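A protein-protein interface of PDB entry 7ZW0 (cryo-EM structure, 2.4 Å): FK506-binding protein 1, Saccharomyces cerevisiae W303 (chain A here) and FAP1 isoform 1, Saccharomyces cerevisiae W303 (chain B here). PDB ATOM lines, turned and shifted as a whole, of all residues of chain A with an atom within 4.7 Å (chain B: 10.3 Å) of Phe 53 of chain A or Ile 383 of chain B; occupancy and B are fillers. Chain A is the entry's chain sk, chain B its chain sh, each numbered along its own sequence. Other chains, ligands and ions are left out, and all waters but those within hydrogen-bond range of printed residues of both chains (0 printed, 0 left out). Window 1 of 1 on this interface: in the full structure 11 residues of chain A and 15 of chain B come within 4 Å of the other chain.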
ATOM      1  N   VAL A  29      27.005 -30.072 -38.335  1.00  0.00           N
ATOM      2  CA  VAL A  29      28.282 -30.730 -38.562  1.00  0.00           C
ATOM      3  C   VAL A  29      28.833 -31.220 -37.231  1.00  0.00           C
ATOM      4  O   VAL A  29      28.548 -30.662 -36.161  1.00  0.00           O
ATOM      5  CB  VAL A  29      29.293 -29.798 -39.263  1.00  0.00           C
ATOM      6  CG1 VAL A  29      28.798 -29.432 -40.649  1.00  0.00           C
ATOM      7  CG2 VAL A  29      29.533 -28.546 -38.436  1.00  0.00           C
ATOM      8  N   THR A  30      29.626 -32.287 -37.313  1.00  0.00           N
ATOM      9  CA  THR A  30      30.261 -32.917 -36.165  1.00  0.00           C
ATOM     10  C   THR A  30      31.767 -32.774 -36.322  1.00  0.00           C
ATOM     11  O   THR A  30      32.335 -33.218 -37.325  1.00  0.00           O
ATOM     12  CB  THR A  30      29.861 -34.390 -36.061  1.00  0.00           C
ATOM     13  OG1 THR A  30      28.446 -34.513 -36.247  1.00  0.00           O
ATOM     14  CG2 THR A  30      30.227 -34.942 -34.706  1.00  0.00           C
ATOM     15  N   ILE A  31      32.409 -32.154 -35.333  1.00  0.00           N
ATOM     16  CA  ILE A  31      33.798 -31.730 -35.420  1.00  0.00           C
ATOM     17  C   ILE A  31      34.580 -32.363 -34.279  1.00  0.00           C
ATOM     18  O   ILE A  31      34.123 -32.367 -33.130  1.00  0.00           O
ATOM     19  CB  ILE A  31      33.923 -30.193 -35.365  1.00  0.00           C
ATOM     20  CG1 ILE A  31      33.098 -29.525 -36.468  1.00  0.00           C
ATOM     21  CG2 ILE A  31      35.374 -29.753 -35.488  1.00  0.00           C
ATOM     22  CD1 ILE A  31      33.359 -30.071 -37.855  1.00  0.00           C
ATOM     23  N   TYR A  33      38.256 -31.356 -32.928  1.00  0.00           N
ATOM     24  CA  TYR A  33      39.183 -30.255 -33.129  1.00  0.00           C
ATOM     25  C   TYR A  33      40.002 -30.039 -31.866  1.00  0.00           C
ATOM     26  O   TYR A  33      39.579 -30.378 -30.758  1.00  0.00           O
ATOM     27  CB  TYR A  33      38.444 -28.963 -33.509  1.00  0.00           C
ATOM     28  CG  TYR A  33      37.735 -28.295 -32.347  1.00  0.00           C
ATOM     29  CD1 TYR A  33      36.522 -28.784 -31.878  1.00  0.00           C
ATOM     30  CD2 TYR A  33      38.276 -27.176 -31.721  1.00  0.00           C
ATOM     31  CE1 TYR A  33      35.868 -28.183 -30.816  1.00  0.00           C
ATOM     32  CE2 TYR A  33      37.630 -26.569 -30.658  1.00  0.00           C
ATOM     33  CZ  TYR A  33      36.427 -27.076 -30.211  1.00  0.00           C
ATOM     34  OH  TYR A  33      35.779 -26.477 -29.156  1.00  0.00           O
ATOM     35  N   ARG A  49      38.527 -33.295 -24.485  1.00  0.00           N
ATOM     36  CA  ARG A  49      37.224 -33.392 -23.837  1.00  0.00           C
ATOM     37  C   ARG A  49      36.548 -34.740 -24.057  1.00  0.00           C
ATOM     38  O   ARG A  49      35.727 -35.143 -23.226  1.00  0.00           O
ATOM     39  CB  ARG A  49      36.301 -32.275 -24.332  1.00  0.00           C
ATOM     40  CG  ARG A  49      36.691 -30.887 -23.855  1.00  0.00           C
ATOM     41  CD  ARG A  49      35.550 -29.898 -24.036  1.00  0.00           C
ATOM     42  NE  ARG A  49      35.022 -29.905 -25.394  1.00  0.00           N
ATOM     43  CZ  ARG A  49      35.443 -29.105 -26.364  1.00  0.00           C
ATOM     44  NH1 ARG A  49      36.422 -28.238 -26.167  1.00  0.00           N
ATOM     45  NH2 ARG A  49      34.868 -29.178 -27.561  1.00  0.00           N
ATOM     46  N   SER A  51      34.376 -35.527 -26.283  1.00  0.00           N
ATOM     47  CA  SER A  51      33.031 -35.387 -26.819  1.00  0.00           C
ATOM     48  C   SER A  51      33.076 -34.600 -28.122  1.00  0.00           C
ATOM     49  O   SER A  51      33.673 -33.516 -28.171  1.00  0.00           O
ATOM     50  CB  SER A  51      32.112 -34.698 -25.808  1.00  0.00           C
ATOM     51  OG  SER A  51      32.702 -33.510 -25.311  1.00  0.00           O
ATOM     52  N   PRO A  52      32.486 -35.121 -29.197  1.00  0.00           N
ATOM     53  CA  PRO A  52      32.471 -34.381 -30.463  1.00  0.00           C
ATOM     54  C   PRO A  52      31.632 -33.116 -30.359  1.00  0.00           C
ATOM     55  O   PRO A  52      30.662 -33.046 -29.601  1.00  0.00           O
ATOM     56  CB  PRO A  52      31.856 -35.378 -31.453  1.00  0.00           C
ATOM     57  CG  PRO A  52      31.993 -36.716 -30.807  1.00  0.00           C
ATOM     58  CD  PRO A  52      31.917 -36.472 -29.335  1.00  0.00           C
ATOM     59  N   PHE A  53      32.024 -32.105 -31.130  1.00  0.00           N
ATOM     60  CA  PHE A  53      31.355 -30.814 -31.116  1.00  0.00           C
ATOM     61  C   PHE A  53      30.398 -30.714 -32.296  1.00  0.00           C
ATOM     62  O   PHE A  53      30.828 -30.691 -33.452  1.00  0.00           O
ATOM     63  CB  PHE A  53      32.397 -29.696 -31.156  1.00  0.00           C
ATOM     64  CG  PHE A  53      31.829 -28.336 -31.417  1.00  0.00           C
ATOM     65  CD1 PHE A  53      31.075 -27.686 -30.457  1.00  0.00           C
ATOM     66  CD2 PHE A  53      32.094 -27.684 -32.611  1.00  0.00           C
ATOM     67  CE1 PHE A  53      30.563 -26.425 -30.698  1.00  0.00           C
ATOM     68  CE2 PHE A  53      31.592 -26.421 -32.853  1.00  0.00           C
ATOM     69  CZ  PHE A  53      30.829 -25.790 -31.892  1.00  0.00           C
ATOM     70  N   GLN A  54      29.103 -30.665 -32.002  1.00  0.00           N
ATOM     71  CA  GLN A  54      28.067 -30.594 -33.022  1.00  0.00           C
ATOM     72  C   GLN A  54      27.528 -29.175 -33.083  1.00  0.00           C
ATOM     73  O   GLN A  54      27.154 -28.605 -32.051  1.00  0.00           O
ATOM     74  CB  GLN A  54      26.932 -31.579 -32.731  1.00  0.00           C
ATOM     75  CG  GLN A  54      27.222 -33.004 -33.166  1.00  0.00           C
ATOM     76  CD  GLN A  54      25.981 -33.873 -33.167  1.00  0.00           C
ATOM     77  OE1 GLN A  54      24.951 -33.505 -32.605  1.00  0.00           O
ATOM     78  NE2 GLN A  54      26.074 -35.034 -33.801  1.00  0.00           N
ATOM     79  N   CYS A  55      27.490 -28.608 -34.286  1.00  0.00           N
ATOM     80  CA  CYS A  55      27.045 -27.227 -34.423  1.00  0.00           C
ATOM     81  C   CYS A  55      26.464 -26.994 -35.807  1.00  0.00           C
ATOM     82  O   CYS A  55      26.773 -27.707 -36.762  1.00  0.00           O
ATOM     83  CB  CYS A  55      28.190 -26.239 -34.183  1.00  0.00           C
ATOM     84  SG  CYS A  55      29.358 -26.127 -35.560  1.00  0.00           S
ATOM     85  N   VAL A  62      29.327 -19.934 -34.460  1.00  0.00           N
ATOM     86  CA  VAL A  62      30.755 -20.082 -34.228  1.00  0.00           C
ATOM     87  C   VAL A  62      31.476 -18.934 -34.922  1.00  0.00           C
ATOM     88  O   VAL A  62      30.857 -18.004 -35.440  1.00  0.00           O
ATOM     89  CB  VAL A  62      31.298 -21.440 -34.720  1.00  0.00           C
ATOM     90  CG1 VAL A  62      30.730 -22.577 -33.883  1.00  0.00           C
ATOM     91  CG2 VAL A  62      30.972 -21.637 -36.188  1.00  0.00           C
ATOM     92  N   TRP A  66      35.746 -20.553 -38.867  1.00  0.00           N
ATOM     93  CA  TRP A  66      35.088 -21.851 -38.983  1.00  0.00           C
ATOM     94  C   TRP A  66      33.937 -21.798 -39.977  1.00  0.00           C
ATOM     95  O   TRP A  66      33.748 -22.733 -40.764  1.00  0.00           O
ATOM     96  CB  TRP A  66      34.587 -22.322 -37.616  1.00  0.00           C
ATOM     97  CG  TRP A  66      35.664 -22.817 -36.704  1.00  0.00           C
ATOM     98  CD1 TRP A  66      36.989 -22.958 -36.998  1.00  0.00           C
ATOM     99  CD2 TRP A  66      35.505 -23.252 -35.349  1.00  0.00           C
ATOM    100  NE1 TRP A  66      37.666 -23.446 -35.907  1.00  0.00           N
ATOM    101  CE2 TRP A  66      36.777 -23.636 -34.882  1.00  0.00           C
ATOM    102  CE3 TRP A  66      34.411 -23.351 -34.485  1.00  0.00           C
ATOM    103  CZ2 TRP A  66      36.985 -24.111 -33.589  1.00  0.00           C
ATOM    104  CZ3 TRP A  66      34.619 -23.823 -33.200  1.00  0.00           C
ATOM    105  CH2 TRP A  66      35.895 -24.197 -32.765  1.00  0.00           C
ATOM    106  N   LEU B 360      24.357 -13.962 -19.249  1.00  0.00           N
ATOM    107  CA  LEU B 360      23.881 -14.412 -20.552  1.00  0.00           C
ATOM    108  C   LEU B 360      22.362 -14.363 -20.613  1.00  0.00           C
ATOM    109  O   LEU B 360      21.697 -14.340 -19.578  1.00  0.00           O
ATOM    110  CB  LEU B 360      24.387 -15.818 -20.866  1.00  0.00           C
ATOM    111  CG  LEU B 360      25.559 -15.881 -21.843  1.00  0.00           C
ATOM    112  CD1 LEU B 360      25.223 -15.112 -23.110  1.00  0.00           C
ATOM    113  CD2 LEU B 360      26.843 -15.364 -21.215  1.00  0.00           C
ATOM    114  N   CYS B 362      20.506 -16.750 -21.623  1.00  0.00           N
ATOM    115  CA  CYS B 362      20.109 -18.022 -21.025  1.00  0.00           C
ATOM    116  C   CYS B 362      20.257 -17.953 -19.512  1.00  0.00           C
ATOM    117  O   CYS B 362      19.412 -18.466 -18.779  1.00  0.00           O
ATOM    118  CB  CYS B 362      20.942 -19.170 -21.597  1.00  0.00           C
ATOM    119  SG  CYS B 362      22.723 -19.029 -21.325  1.00  0.00           S
ATOM    120  N   LYS B 364      22.592 -19.375 -17.788  1.00  0.00           N
ATOM    121  CA  LYS B 364      23.300 -20.542 -17.269  1.00  0.00           C
ATOM    122  C   LYS B 364      24.647 -20.119 -16.719  1.00  0.00           C
ATOM    123  O   LYS B 364      25.073 -20.600 -15.669  1.00  0.00           O
ATOM    124  CB  LYS B 364      23.494 -21.596 -18.364  1.00  0.00           C
ATOM    125  CG  LYS B 364      22.355 -22.595 -18.504  1.00  0.00           C
ATOM    126  CD  LYS B 364      21.106 -21.962 -19.093  1.00  0.00           C
ATOM    127  CE  LYS B 364      19.990 -22.977 -19.267  1.00  0.00           C
ATOM    128  NZ  LYS B 364      18.774 -22.349 -19.853  1.00  0.00           N
ATOM    129  N   HIS B 365      25.310 -19.210 -17.417  1.00  0.00           N
ATOM    130  CA  HIS B 365      26.599 -18.730 -16.955  1.00  0.00           C
ATOM    131  C   HIS B 365      26.720 -17.241 -17.159  1.00  0.00           C
ATOM    132  O   HIS B 365      25.914 -16.642 -17.873  1.00  0.00           O
ATOM    133  CB  HIS B 365      27.732 -19.447 -17.694  1.00  0.00           C
ATOM    134  CG  HIS B 365      27.445 -19.703 -19.141  1.00  0.00           C
ATOM    135  ND1 HIS B 365      27.433 -20.969 -19.683  1.00  0.00           N
ATOM    136  CD2 HIS B 365      27.148 -18.857 -20.156  1.00  0.00           C
ATOM    137  CE1 HIS B 365      27.151 -20.892 -20.971  1.00  0.00           C
ATOM    138  NE2 HIS B 365      26.970 -19.622 -21.282  1.00  0.00           N
ATOM    139  N   PRO B 368      33.150 -15.275 -19.290  1.00  0.00           N
ATOM    140  CA  PRO B 368      34.592 -15.300 -19.057  1.00  0.00           C
ATOM    141  C   PRO B 368      35.353 -14.515 -20.111  1.00  0.00           C
ATOM    142  O   PRO B 368      36.569 -14.517 -20.071  1.00  0.00           O
ATOM    143  CB  PRO B 368      34.940 -16.792 -19.138  1.00  0.00           C
ATOM    144  CG  PRO B 368      33.711 -17.497 -19.631  1.00  0.00           C
ATOM    145  CD  PRO B 368      32.695 -16.468 -20.018  1.00  0.00           C
ATOM    146  N   PHE B 369      34.654 -13.877 -21.043  1.00  0.00           N
ATOM    147  CA  PHE B 369      35.297 -13.083 -22.085  1.00  0.00           C
ATOM    148  C   PHE B 369      35.935 -11.836 -21.498  1.00  0.00           C
ATOM    149  O   PHE B 369      35.498 -11.352 -20.461  1.00  0.00           O
ATOM    150  CB  PHE B 369      34.272 -12.654 -23.137  1.00  0.00           C
ATOM    151  CG  PHE B 369      33.433 -13.780 -23.665  1.00  0.00           C
ATOM    152  CD1 PHE B 369      33.859 -14.531 -24.742  1.00  0.00           C
ATOM    153  CD2 PHE B 369      32.208 -14.076 -23.095  1.00  0.00           C
ATOM    154  CE1 PHE B 369      33.086 -15.566 -25.228  1.00  0.00           C
ATOM    155  CE2 PHE B 369      31.430 -15.108 -23.577  1.00  0.00           C
ATOM    156  CZ  PHE B 369      31.870 -15.857 -24.647  1.00  0.00           C
ATOM    157  N   GLU B 378      24.327 -13.261 -27.406  1.00  0.00           N
ATOM    158  CA  GLU B 378      23.538 -14.411 -26.965  1.00  0.00           C
ATOM    159  C   GLU B 378      24.116 -15.766 -27.381  1.00  0.00           C
ATOM    160  O   GLU B 378      24.132 -16.693 -26.574  1.00  0.00           O
ATOM    161  CB  GLU B 378      22.067 -14.269 -27.378  1.00  0.00           C
ATOM    162  CG  GLU B 378      21.415 -12.993 -26.873  1.00  0.00           C
ATOM    163  CD  GLU B 378      19.943 -12.915 -27.219  1.00  0.00           C
ATOM    164  OE1 GLU B 378      19.322 -11.865 -26.949  1.00  0.00           O
ATOM    165  OE2 GLU B 378      19.406 -13.904 -27.760  1.00  0.00           O
ATOM    166  N   PRO B 379      24.594 -15.900 -28.638  1.00  0.00           N
ATOM    167  CA  PRO B 379      25.251 -17.178 -28.947  1.00  0.00           C
ATOM    168  C   PRO B 379      26.520 -17.292 -28.121  1.00  0.00           C
ATOM    169  O   PRO B 379      27.214 -16.292 -27.936  1.00  0.00           O
ATOM    170  CB  PRO B 379      25.590 -17.066 -30.440  1.00  0.00           C
ATOM    171  CG  PRO B 379      25.287 -15.660 -30.836  1.00  0.00           C
ATOM    172  CD  PRO B 379      24.252 -15.174 -29.873  1.00  0.00           C
ATOM    173  N   CYS B 380      26.835 -18.484 -27.633  1.00  0.00           N
ATOM    174  CA  CYS B 380      27.987 -18.627 -26.751  1.00  0.00           C
ATOM    175  C   CYS B 380      29.114 -19.443 -27.354  1.00  0.00           C
ATOM    176  O   CYS B 380      28.891 -20.557 -27.818  1.00  0.00           O
ATOM    177  CB  CYS B 380      27.543 -19.281 -25.443  1.00  0.00           C
ATOM    178  SG  CYS B 380      26.135 -18.490 -24.639  1.00  0.00           S
ATOM    179  N   LEU B 381      30.327 -18.904 -27.351  1.00  0.00           N
ATOM    180  CA  LEU B 381      31.464 -19.686 -27.822  1.00  0.00           C
ATOM    181  C   LEU B 381      31.551 -20.825 -26.835  1.00  0.00           C
ATOM    182  O   LEU B 381      31.877 -21.954 -27.205  1.00  0.00           O
ATOM    183  CB  LEU B 381      32.741 -18.855 -27.802  1.00  0.00           C
ATOM    184  CG  LEU B 381      32.676 -17.524 -28.554  1.00  0.00           C
ATOM    185  CD1 LEU B 381      33.952 -16.723 -28.343  1.00  0.00           C
ATOM    186  CD2 LEU B 381      32.416 -17.754 -30.035  1.00  0.00           C
ATOM    187  N   GLN B 382      31.256 -20.534 -25.571  1.00  0.00           N
ATOM    188  CA  GLN B 382      31.226 -21.576 -24.549  1.00  0.00           C
ATOM    189  C   GLN B 382      30.154 -22.622 -24.835  1.00  0.00           C
ATOM    190  O   GLN B 382      28.961 -22.315 -24.837  1.00  0.00           O
ATOM    191  CB  GLN B 382      31.030 -20.958 -23.163  1.00  0.00           C
ATOM    192  CG  GLN B 382      30.254 -19.651 -23.169  1.00  0.00           C
ATOM    193  CD  GLN B 382      30.274 -18.950 -21.825  1.00  0.00           C
ATOM    194  OE1 GLN B 382      30.495 -19.575 -20.788  1.00  0.00           O
ATOM    195  NE2 GLN B 382      30.041 -17.643 -21.836  1.00  0.00           N
ATOM    196  N   ILE B 383      30.577 -23.858 -25.083  1.00  0.00           N
ATOM    197  CA  ILE B 383      29.633 -24.937 -25.370  1.00  0.00           C
ATOM    198  C   ILE B 383      29.195 -25.684 -24.117  1.00  0.00           C
ATOM    199  O   ILE B 383      30.014 -26.008 -23.256  1.00  0.00           O
ATOM    200  CB  ILE B 383      30.209 -25.926 -26.404  1.00  0.00           C
ATOM    201  CG1 ILE B 383      31.628 -26.344 -26.019  1.00  0.00           C
ATOM    202  CG2 ILE B 383      30.237 -25.298 -27.786  1.00  0.00           C
ATOM    203  CD1 ILE B 383      32.310 -27.208 -27.056  1.00  0.00           C
ATOM    204  N   ASP B 384      27.898 -25.940 -24.001  1.00  0.00           N
ATOM    205  CA  ASP B 384      27.381 -26.627 -22.824  1.00  0.00           C
ATOM    206  C   ASP B 384      27.066 -28.075 -23.159  1.00  0.00           C
ATOM    207  O   ASP B 384      26.343 -28.354 -24.113  1.00  0.00           O
ATOM    208  CB  ASP B 384      26.127 -25.920 -22.309  1.00  0.00           C
ATOM    209  CG  ASP B 384      25.764 -26.326 -20.893  1.00  0.00           C
ATOM    210  OD1 ASP B 384      26.612 -26.933 -20.206  1.00  0.00           O
ATOM    211  OD2 ASP B 384      24.628 -26.035 -20.466  1.00  0.00           O
ATOM    212  N   SER B 385      27.602 -29.000 -22.371  1.00  0.00           N
ATOM    213  CA  SER B 385      27.386 -30.421 -22.627  1.00  0.00           C
ATOM    214  C   SER B 385      25.931 -30.837 -22.445  1.00  0.00           C
ATOM    215  O   SER B 385      25.372 -30.684 -21.359  1.00  0.00           O
ATOM    216  CB  SER B 385      28.287 -31.253 -21.715  1.00  0.00           C
ATOM    217  OG  SER B 385      29.653 -30.954 -21.940  1.00  0.00           O
ATOM    218  N   VAL B 386      25.316 -31.363 -23.503  1.00  0.00           N
ATOM    219  CA  VAL B 386      23.926 -31.809 -23.424  1.00  0.00           C
ATOM    220  C   VAL B 386      23.878 -33.290 -23.785  1.00  0.00           C
ATOM    221  O   VAL B 386      24.417 -33.694 -24.812  1.00  0.00           O
ATOM    222  CB  VAL B 386      23.012 -31.010 -24.380  1.00  0.00           C
ATOM    223  CG1 VAL B 386      21.598 -31.571 -24.370  1.00  0.00           C
ATOM    224  CG2 VAL B 386      22.990 -29.537 -24.002  1.00  0.00           C
ATOM    225  N   THR B 394      27.194 -37.690 -24.842  1.00  0.00           N
ATOM    226  CA  THR B 394      26.982 -36.293 -24.492  1.00  0.00           C
ATOM    227  C   THR B 394      27.572 -35.417 -25.577  1.00  0.00           C
ATOM    228  O   THR B 394      28.765 -35.493 -25.864  1.00  0.00           O
ATOM    229  CB  THR B 394      27.666 -35.956 -23.155  1.00  0.00           C
ATOM    230  OG1 THR B 394      27.303 -36.931 -22.170  1.00  0.00           O
ATOM    231  CG2 THR B 394      27.254 -34.580 -22.677  1.00  0.00           C
ATOM    232  N   PHE B 395      26.739 -34.587 -26.187  1.00  0.00           N
ATOM    233  CA  PHE B 395      27.218 -33.703 -27.234  1.00  0.00           C
ATOM    234  C   PHE B 395      27.216 -32.282 -26.712  1.00  0.00           C
ATOM    235  O   PHE B 395      26.188 -31.779 -26.266  1.00  0.00           O
ATOM    236  CB  PHE B 395      26.334 -33.817 -28.474  1.00  0.00           C
ATOM    237  CG  PHE B 395      26.347 -35.181 -29.103  1.00  0.00           C
ATOM    238  CD1 PHE B 395      27.287 -35.502 -30.065  1.00  0.00           C
ATOM    239  CD2 PHE B 395      25.423 -36.142 -28.729  1.00  0.00           C
ATOM    240  CE1 PHE B 395      27.305 -36.755 -30.645  1.00  0.00           C
ATOM    241  CE2 PHE B 395      25.434 -37.396 -29.304  1.00  0.00           C
ATOM    242  CZ  PHE B 395      26.377 -37.704 -30.263  1.00  0.00           C
ATOM    243  N   SER B 396      28.376 -31.631 -26.751  1.00  0.00           N
ATOM    244  CA  SER B 396      28.487 -30.264 -26.248  1.00  0.00           C
ATOM    245  C   SER B 396      28.036 -29.256 -27.288  1.00  0.00           C
ATOM    246  O   SER B 396      28.643 -29.143 -28.352  1.00  0.00           O
ATOM    247  CB  SER B 396      29.922 -29.969 -25.816  1.00  0.00           C
ATOM    248  OG  SER B 396      30.357 -30.892 -24.833  1.00  0.00           O
ATOM    249  N   VAL B 397      26.976 -28.516 -26.983  1.00  0.00           N
ATOM    250  CA  VAL B 397      26.445 -27.543 -27.932  1.00  0.00           C
ATOM    251  C   VAL B 397      26.336 -26.160 -27.296  1.00  0.00           C
ATOM    252  O   VAL B 397      26.053 -26.042 -26.107  1.00  0.00           O
ATOM    253  CB  VAL B 397      25.071 -27.988 -28.481  1.00  0.00           C
ATOM    254  CG1 VAL B 397      25.240 -29.032 -29.574  1.00  0.00           C
ATOM    255  CG2 VAL B 397      24.189 -28.515 -27.363  1.00  0.00           C
ATOM    256  N   PRO B 398      26.537 -25.069 -28.088  1.00  0.00           N
ATOM    257  CA  PRO B 398      26.424 -23.782 -27.382  1.00  0.00           C
ATOM    258  C   PRO B 398      25.030 -23.527 -26.825  1.00  0.00           C
ATOM    259  O   PRO B 398      24.052 -24.079 -27.325  1.00  0.00           O
ATOM    260  CB  PRO B 398      26.726 -22.755 -28.476  1.00  0.00           C
ATOM    261  CG  PRO B 398      26.397 -23.442 -29.751  1.00  0.00           C
ATOM    262  CD  PRO B 398      26.834 -24.854 -29.525  1.00  0.00           C
ATOM    263  N   CYS B 399      24.933 -22.684 -25.806  1.00  0.00           N
ATOM    264  CA  CYS B 399      23.625 -22.353 -25.261  1.00  0.00           C
ATOM    265  C   CYS B 399      22.801 -21.635 -26.317  1.00  0.00           C
ATOM    266  O   CYS B 399      23.316 -20.777 -27.035  1.00  0.00           O
ATOM    267  CB  CYS B 399      23.762 -21.493 -24.007  1.00  0.00           C
ATOM    268  SG  CYS B 399      24.511 -22.354 -22.606  1.00  0.00           S
ATOM    269  N   GLY B 400      21.521 -21.975 -26.413  1.00  0.00           N
ATOM    270  CA  GLY B 400      20.676 -21.381 -27.433  1.00  0.00           C
ATOM    271  C   GLY B 400      20.579 -22.288 -28.643  1.00  0.00           C
ATOM    272  O   GLY B 400      19.938 -21.936 -29.635  1.00  0.00           O
ATOM    273  N   PHE B 401      21.211 -23.457 -28.571  1.00  0.00           N
ATOM    274  CA  PHE B 401      21.170 -24.407 -29.678  1.00  0.00           C
ATOM    275  C   PHE B 401      19.761 -24.959 -29.837  1.00  0.00           C
ATOM    276  O   PHE B 401      19.135 -25.365 -28.857  1.00  0.00           O
ATOM    277  CB  PHE B 401      22.157 -25.552 -29.445  1.00  0.00           C
ATOM    278  CG  PHE B 401      22.046 -26.666 -30.446  1.00  0.00           C
ATOM    279  CD1 PHE B 401      22.510 -26.502 -31.739  1.00  0.00           C
ATOM    280  CD2 PHE B 401      21.483 -27.883 -30.091  1.00  0.00           C
ATOM    281  CE1 PHE B 401      22.407 -27.524 -32.662  1.00  0.00           C
ATOM    282  CE2 PHE B 401      21.380 -28.908 -31.008  1.00  0.00           C
ATOM    283  CZ  PHE B 401      21.842 -28.729 -32.296  1.00  0.00           C
ATOM    284  N   PRO B 405      20.254 -33.493 -29.221  1.00  0.00           N
ATOM    285  CA  PRO B 405      21.391 -34.173 -29.857  1.00  0.00           C
ATOM    286  C   PRO B 405      21.052 -35.561 -30.380  1.00  0.00           C
ATOM    287  O   PRO B 405      20.292 -36.295 -29.746  1.00  0.00           O
ATOM    288  CB  PRO B 405      22.421 -34.272 -28.726  1.00  0.00           C
ATOM    289  CG  PRO B 405      21.632 -34.130 -27.470  1.00  0.00           C
ATOM    290  CD  PRO B 405      20.519 -33.186 -27.809  1.00  0.00           C
ATOM    291  N   ARG B 406      21.611 -35.915 -31.533  1.00  0.00           N
ATOM    292  CA  ARG B 406      21.333 -37.218 -32.127  1.00  0.00           C
ATOM    293  C   ARG B 406      22.586 -38.078 -32.184  1.00  0.00           C
ATOM    294  O   ARG B 406      23.627 -37.631 -32.666  1.00  0.00           O
ATOM    295  CB  ARG B 406      20.765 -37.045 -33.538  1.00  0.00           C
ATOM    296  CG  ARG B 406      19.568 -36.110 -33.641  1.00  0.00           C
ATOM    297  CD  ARG B 406      18.243 -36.856 -33.576  1.00  0.00           C
ATOM    298  NE  ARG B 406      17.957 -37.393 -32.248  1.00  0.00           N
ATOM    299  CZ  ARG B 406      17.222 -36.776 -31.331  1.00  0.00           C
ATOM    300  NH1 ARG B 406      16.685 -35.592 -31.593  1.00  0.00           N
ATOM    301  NH2 ARG B 406      17.018 -37.347 -30.153  1.00  0.00           N
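The side-chain hydroxyl (OG1) of Thr 30 of chain A sits at hydrogen-bond distance from the side-chain amide nitrogen (NE2) of Gln 54 of chain A, at 3.4 Å. N of Ile 31 of chain A lies within hydrogen-bond range of O of Phe 53 of chain A. The side-chain hydroxyl (OH) of Tyr 33 of chain A sits at hydrogen-bond distance from the guanidinium group (NH2) of Arg 49 of chain A (3.3 Å). The backbone carbonyl oxygen of Val 397 of chain B sits at hydrogen-bond distance from the backbone NH of Asp 384 of chain B, 2.8 Å away. The side-chain hydroxyl (OG) of Ser 385 of chain B sits at hydrogen-bond distance from the side-chain hydroxyl (OG) of Ser 396 of chain B (3.0 Å). N of Phe 395 of chain B sits at hydrogen-bond distance from O of Val 386 of chain B (2.8 Å).
Among the printed residues, pairs that only touch across the chains: Arg 49 of chain A with Ile 383 of chain B (3.3 Å), Ser 51 of chain A with Thr 394 of chain B (3.4 Å), Ser 51 of chain A with Ser 396 of chain B (3.5 Å), Pro 52 of chain A with Ser 396 of chain B (3.9 Å), Phe 53 of chain A with Ile 383 of chain B (3.1 Å), Phe 53 of chain A with Ser 396 of chain B (3.5 Å), Gln 54 of chain A with Phe 395 of chain B (3.7 Å), Gln 54 of chain A with Ser 396 of chain B (3.98 Å), Gln 54 of chain A with Val 397 of chain B (3.2 Å) and Gln 54 of chain A with Arg 406 of chain B (3.7 Å).
Of the printed residues of chain B, Phe 53 of chain A touches Ile 383 and Ser 396. Ile 383 of chain B touches two residues of chain A. No residue of chain B comes within 4 Å of Ile 31 of chain A. Pro 52 of chain A touches just one residue of chain B: Ser 396. Of the printed residues of chain A, Arg 406 of chain B touches Gln 54 (3.7 Å). Of the printed residues of chain A, Val 397 of chain B touches Gln 54. Of the printed residues of chain A, Ser 396 of chain B touches Ser 51 (3.5 Å), Pro 52 (3.9 Å), Phe 53 (3.5 Å) and Gln 54 (3.98 Å). Of the printed residues of chain B, Gln 54 of chain A touches Phe 395 (3.7 Å), Ser 396 (3.98 Å), Val 397 (3.2 Å) and Arg 406 (3.7 Å). Gln 382 of chain B touches none of the printed residues of chain A. Pro 398 of chain B touches none of the printed residues of chain A. The nearest residue of chain B that does not touch Phe 53 of chain A is Pro 398 of chain B (4.2 Å). The nearest printed residue of chain A that does not touch Ser 396 of chain B is Arg 49 of chain A (4.8 Å).
Printed residues of chain A that touch a printed residue of chain B: Arg 49, Ser 51, Pro 52, Phe 53 and Gln 54. Hydrophobic or aromatic side chains of chain A within 4 Å of the printed part of chain B: Phe 53. Hydrophobic or aromatic side chains of chain B within 4 Å of the printed part of chain A: Ile 383, Phe 395 and Val 397. Among the printed residues, no Asp or Glu carboxylate lies within 4 Å of a Lys or Arg side-chain nitrogen of the other chain.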
